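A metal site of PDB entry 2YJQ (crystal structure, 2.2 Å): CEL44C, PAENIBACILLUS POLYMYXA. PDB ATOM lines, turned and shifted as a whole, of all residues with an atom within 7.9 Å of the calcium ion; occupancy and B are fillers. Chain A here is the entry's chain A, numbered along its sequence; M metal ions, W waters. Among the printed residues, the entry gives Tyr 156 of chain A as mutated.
The backbone NH (N) of Asn 153 is in hydrogen-bond range of the side-chain carboxylate (OD1) of Asp 151, 2.9 Å away. The side-chain amide oxygen of Asn 54 is in hydrogen-bond range of the backbone NH of Glu 56, at 2.8 Å.
Four residues have an atom within 4 Å of the calcium ion: Glu 56, Asp 151, Asp 154 and Tyr 156.
The calcium ion is bound by the backbone carbonyl oxygen (O) of Asp 151, the backbone carbonyl oxygen (O) of Tyr 156, water W2, the side-chain carboxylate (OE2) of Glu 56, water W1, the side-chain carboxylate (OE1) of Glu 56 and the side-chain carboxylate (OD1) of Asp 154.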
ATOM      1  N   ASN A  54       6.404  -1.268 -22.179  1.00  0.00           N
ATOM      2  CA  ASN A  54       4.962  -1.508 -22.163  1.00  0.00           C
ATOM      3  C   ASN A  54       4.589  -2.360 -23.387  1.00  0.00           C
ATOM      4  O   ASN A  54       4.621  -1.847 -24.509  1.00  0.00           O
ATOM      5  CB  ASN A  54       4.256  -0.120 -22.192  1.00  0.00           C
ATOM      6  CG  ASN A  54       2.710  -0.209 -22.334  1.00  0.00           C
ATOM      7  OD1 ASN A  54       2.110  -1.264 -22.750  1.00  0.00           O
ATOM      8  ND2 ASN A  54       2.035   0.961 -22.054  1.00  0.00           N
ATOM      9  N   TRP A  55       4.253  -3.629 -23.243  1.00  0.00           N
ATOM     10  CA  TRP A  55       4.023  -4.404 -24.466  1.00  0.00           C
ATOM     11  C   TRP A  55       2.850  -3.913 -25.341  1.00  0.00           C
ATOM     12  O   TRP A  55       2.791  -4.236 -26.549  1.00  0.00           O
ATOM     13  CB  TRP A  55       3.798  -5.882 -24.168  1.00  0.00           C
ATOM     14  CG  TRP A  55       2.427  -6.205 -23.661  1.00  0.00           C
ATOM     15  CD1 TRP A  55       2.002  -6.065 -22.394  1.00  0.00           C
ATOM     16  CD2 TRP A  55       1.314  -6.818 -24.394  1.00  0.00           C
ATOM     17  NE1 TRP A  55       0.687  -6.489 -22.266  1.00  0.00           N
ATOM     18  CE2 TRP A  55       0.248  -6.985 -23.466  1.00  0.00           C
ATOM     19  CE3 TRP A  55       1.126  -7.258 -25.732  1.00  0.00           C
ATOM     20  CZ2 TRP A  55      -0.994  -7.545 -23.812  1.00  0.00           C
ATOM     21  CZ3 TRP A  55      -0.095  -7.814 -26.100  1.00  0.00           C
ATOM     22  CH2 TRP A  55      -1.162  -7.953 -25.131  1.00  0.00           C
ATOM     23  N   GLU A  56       1.916  -3.139 -24.771  1.00  0.00           N
ATOM     24  CA  GLU A  56       0.762  -2.770 -25.568  1.00  0.00           C
ATOM     25  C   GLU A  56       1.121  -1.787 -26.630  1.00  0.00           C
ATOM     26  O   GLU A  56       0.527  -1.806 -27.678  1.00  0.00           O
ATOM     27  CB  GLU A  56      -0.394  -2.182 -24.722  1.00  0.00           C
ATOM     28  CG  GLU A  56      -0.889  -3.112 -23.597  1.00  0.00           C
ATOM     29  CD  GLU A  56      -1.944  -2.453 -22.706  1.00  0.00           C
ATOM     30  OE1 GLU A  56      -2.085  -1.183 -22.747  1.00  0.00           O
ATOM     31  OE2 GLU A  56      -2.657  -3.195 -21.965  1.00  0.00           O
ATOM     32  N   ASN A 136       1.522   3.791 -17.114  1.00  0.00           N
ATOM     33  CA  ASN A 136       0.450   2.816 -16.887  1.00  0.00           C
ATOM     34  C   ASN A 136       0.828   1.878 -15.767  1.00  0.00           C
ATOM     35  O   ASN A 136       2.015   1.598 -15.582  1.00  0.00           O
ATOM     36  CB  ASN A 136       0.117   2.022 -18.143  1.00  0.00           C
ATOM     37  CG  ASN A 136      -0.529   2.869 -19.190  1.00  0.00           C
ATOM     38  OD1 ASN A 136      -1.345   3.712 -18.864  1.00  0.00           O
ATOM     39  ND2 ASN A 136      -0.176   2.675 -20.461  1.00  0.00           N
ATOM     40  N   GLN A 137      -0.165   1.415 -15.002  1.00  0.00           N
ATOM     41  CA  GLN A 137       0.139   0.514 -13.883  1.00  0.00           C
ATOM     42  C   GLN A 137       0.223  -0.977 -14.333  1.00  0.00           C
ATOM     43  O   GLN A 137      -0.669  -1.484 -15.010  1.00  0.00           O
ATOM     44  CB  GLN A 137      -0.953   0.637 -12.840  1.00  0.00           C
ATOM     45  CG  GLN A 137      -0.595   0.121 -11.496  1.00  0.00           C
ATOM     46  CD  GLN A 137      -1.812   0.170 -10.500  1.00  0.00           C
ATOM     47  OE1 GLN A 137      -1.972  -0.761  -9.705  1.00  0.00           O
ATOM     48  NE2 GLN A 137      -2.655   1.245 -10.546  1.00  0.00           N
ATOM     49  N   GLN A 147      -7.430 -10.408 -23.855  1.00  0.00           N
ATOM     50  CA  GLN A 147      -7.642  -9.849 -25.152  1.00  0.00           C
ATOM     51  C   GLN A 147      -6.310  -9.968 -25.872  1.00  0.00           C
ATOM     52  O   GLN A 147      -5.287  -9.558 -25.308  1.00  0.00           O
ATOM     53  CB  GLN A 147      -8.074  -8.401 -25.009  1.00  0.00           C
ATOM     54  CG  GLN A 147      -9.525  -8.135 -24.477  1.00  0.00           C
ATOM     55  CD  GLN A 147      -9.676  -6.699 -23.984  1.00  0.00           C
ATOM     56  OE1 GLN A 147      -9.618  -6.430 -22.780  1.00  0.00           O
ATOM     57  NE2 GLN A 147      -9.807  -5.761 -24.905  1.00  0.00           N
ATOM     58  N   PRO A 150      -4.894  -5.795 -26.690  1.00  0.00           N
ATOM     59  CA  PRO A 150      -5.169  -5.256 -25.353  1.00  0.00           C
ATOM     60  C   PRO A 150      -5.845  -3.899 -25.411  1.00  0.00           C
ATOM     61  O   PRO A 150      -5.765  -3.174 -26.404  1.00  0.00           O
ATOM     62  CB  PRO A 150      -3.798  -5.110 -24.719  1.00  0.00           C
ATOM     63  CG  PRO A 150      -2.883  -4.879 -25.930  1.00  0.00           C
ATOM     64  CD  PRO A 150      -3.456  -5.719 -27.029  1.00  0.00           C
ATOM     65  N   ASP A 151      -6.545  -3.578 -24.340  1.00  0.00           N
ATOM     66  CA  ASP A 151      -7.144  -2.266 -24.178  1.00  0.00           C
ATOM     67  C   ASP A 151      -6.066  -1.209 -24.001  1.00  0.00           C
ATOM     68  O   ASP A 151      -5.412  -1.181 -22.944  1.00  0.00           O
ATOM     69  CB  ASP A 151      -8.051  -2.278 -22.947  1.00  0.00           C
ATOM     70  CG  ASP A 151      -8.962  -1.079 -22.888  1.00  0.00           C
ATOM     71  OD1 ASP A 151      -8.715  -0.047 -23.588  1.00  0.00           O
ATOM     72  OD2 ASP A 151      -9.957  -1.185 -22.149  1.00  0.00           O
ATOM     73  N   LEU A 152      -5.910  -0.372 -25.018  1.00  0.00           N
ATOM     74  CA  LEU A 152      -4.968   0.734 -25.053  1.00  0.00           C
ATOM     75  C   LEU A 152      -5.471   1.999 -24.320  1.00  0.00           C
ATOM     76  O   LEU A 152      -4.736   2.981 -24.203  1.00  0.00           O
ATOM     77  CB  LEU A 152      -4.686   1.164 -26.514  1.00  0.00           C
ATOM     78  CG  LEU A 152      -4.175   0.123 -27.524  1.00  0.00           C
ATOM     79  CD1 LEU A 152      -4.050   0.700 -28.962  1.00  0.00           C
ATOM     80  CD2 LEU A 152      -2.849  -0.550 -27.051  1.00  0.00           C
ATOM     81  N   ASN A 153      -6.730   1.986 -23.900  1.00  0.00           N
ATOM     82  CA  ASN A 153      -7.366   3.194 -23.373  1.00  0.00           C
ATOM     83  C   ASN A 153      -7.470   3.278 -21.864  1.00  0.00           C
ATOM     84  O   ASN A 153      -7.700   4.390 -21.329  1.00  0.00           O
ATOM     85  CB  ASN A 153      -8.718   3.463 -24.077  1.00  0.00           C
ATOM     86  CG  ASN A 153      -8.547   3.771 -25.591  1.00  0.00           C
ATOM     87  OD1 ASN A 153      -9.282   3.273 -26.408  1.00  0.00           O
ATOM     88  ND2 ASN A 153      -7.542   4.549 -25.940  1.00  0.00           N
ATOM     89  N   ASP A 154      -7.246   2.157 -21.168  1.00  0.00           N
ATOM     90  CA  ASP A 154      -7.265   2.156 -19.688  1.00  0.00           C
ATOM     91  C   ASP A 154      -5.904   2.541 -19.093  1.00  0.00           C
ATOM     92  O   ASP A 154      -4.964   2.908 -19.808  1.00  0.00           O
ATOM     93  CB  ASP A 154      -7.779   0.803 -19.115  1.00  0.00           C
ATOM     94  CG  ASP A 154      -6.819  -0.352 -19.390  1.00  0.00           C
ATOM     95  OD1 ASP A 154      -5.696  -0.072 -19.846  1.00  0.00           O
ATOM     96  OD2 ASP A 154      -7.190  -1.534 -19.158  1.00  0.00           O
ATOM     97  N   ASN A 155      -5.781   2.405 -17.778  1.00  0.00           N
ATOM     98  CA  ASN A 155      -4.560   2.790 -17.079  1.00  0.00           C
ATOM     99  C   ASN A 155      -3.717   1.603 -16.652  1.00  0.00           C
ATOM    100  O   ASN A 155      -2.846   1.735 -15.736  1.00  0.00           O
ATOM    101  CB  ASN A 155      -4.919   3.689 -15.864  1.00  0.00           C
ATOM    102  CG  ASN A 155      -3.699   4.440 -15.315  1.00  0.00           C
ATOM    103  OD1 ASN A 155      -2.982   5.145 -16.053  1.00  0.00           O
ATOM    104  ND2 ASN A 155      -3.407   4.232 -14.018  1.00  0.00           N
ATOM    105  N   TYR A 156      -3.959   0.455 -17.288  1.00  0.00           N
ATOM    106  CA  TYR A 156      -3.342  -0.807 -16.854  1.00  0.00           C
ATOM    107  C   TYR A 156      -2.596  -1.561 -17.967  1.00  0.00           C
ATOM    108  O   TYR A 156      -2.979  -1.472 -19.135  1.00  0.00           O
ATOM    109  CB  TYR A 156      -4.380  -1.779 -16.278  1.00  0.00           C
ATOM    110  CG  TYR A 156      -5.182  -1.179 -15.189  1.00  0.00           C
ATOM    111  CD1 TYR A 156      -4.629  -0.993 -13.919  1.00  0.00           C
ATOM    112  CD2 TYR A 156      -6.483  -0.704 -15.443  1.00  0.00           C
ATOM    113  CE1 TYR A 156      -5.367  -0.414 -12.908  1.00  0.00           C
ATOM    114  CE2 TYR A 156      -7.231  -0.114 -14.423  1.00  0.00           C
ATOM    115  CZ  TYR A 156      -6.648   0.030 -13.161  1.00  0.00           C
ATOM    116  OH  TYR A 156      -7.372   0.601 -12.169  1.00  0.00           O
ATOM    117  N   VAL A 157      -1.537  -2.273 -17.589  1.00  0.00           N
ATOM    118  CA  VAL A 157      -0.928  -3.279 -18.495  1.00  0.00           C
ATOM    119  C   VAL A 157      -0.934  -4.612 -17.740  1.00  0.00           C
ATOM    120  O   VAL A 157      -0.437  -4.680 -16.603  1.00  0.00           O
ATOM    121  CB  VAL A 157       0.491  -2.905 -18.896  1.00  0.00           C
ATOM    122  CG1 VAL A 157       1.130  -3.979 -19.853  1.00  0.00           C
ATOM    123  CG2 VAL A 157       0.475  -1.567 -19.545  1.00  0.00           C
ATOM    124  N   TYR A 158      -1.555  -5.634 -18.317  1.00  0.00           N
ATOM    125  CA  TYR A 158      -1.613  -6.913 -17.641  1.00  0.00           C
ATOM    126  C   TYR A 158      -0.503  -7.867 -18.097  1.00  0.00           C
ATOM    127  O   TYR A 158      -0.390  -8.186 -19.290  1.00  0.00           O
ATOM    128  CB  TYR A 158      -2.992  -7.542 -17.855  1.00  0.00           C
ATOM    129  CG  TYR A 158      -4.098  -6.702 -17.304  1.00  0.00           C
ATOM    130  CD1 TYR A 158      -4.415  -6.717 -15.925  1.00  0.00           C
ATOM    131  CD2 TYR A 158      -4.812  -5.846 -18.140  1.00  0.00           C
ATOM    132  CE1 TYR A 158      -5.476  -5.901 -15.405  1.00  0.00           C
ATOM    133  CE2 TYR A 158      -5.832  -5.011 -17.640  1.00  0.00           C
ATOM    134  CZ  TYR A 158      -6.134  -5.059 -16.252  1.00  0.00           C
ATOM    135  OH  TYR A 158      -7.116  -4.229 -15.770  1.00  0.00           O
ATOM    136  N   GLU A 161      -1.743 -11.396 -19.211  1.00  0.00           N
ATOM    137  CA  GLU A 161      -2.290 -11.232 -20.575  1.00  0.00           C
ATOM    138  C   GLU A 161      -1.206 -11.220 -21.710  1.00  0.00           C
ATOM    139  O   GLU A 161      -1.449 -11.691 -22.831  1.00  0.00           O
ATOM    140  CB  GLU A 161      -3.108  -9.957 -20.678  1.00  0.00           C
ATOM    141  CG  GLU A 161      -3.845  -9.782 -21.948  1.00  0.00           C
ATOM    142  CD  GLU A 161      -4.771  -8.550 -21.898  1.00  0.00           C
ATOM    143  OE1 GLU A 161      -4.252  -7.425 -21.730  1.00  0.00           O
ATOM    144  OE2 GLU A 161      -6.017  -8.725 -22.022  1.00  0.00           O
HETATM  145 CA    CA M   1      -4.002  -1.348 -21.176  1.00  0.00          CA
HETATM  146  O   HOH W   1      -5.478  -3.142 -20.505  1.00  0.00           O
HETATM  147  O   HOH W   2      -3.300   0.883 -21.238  1.00  0.00           O
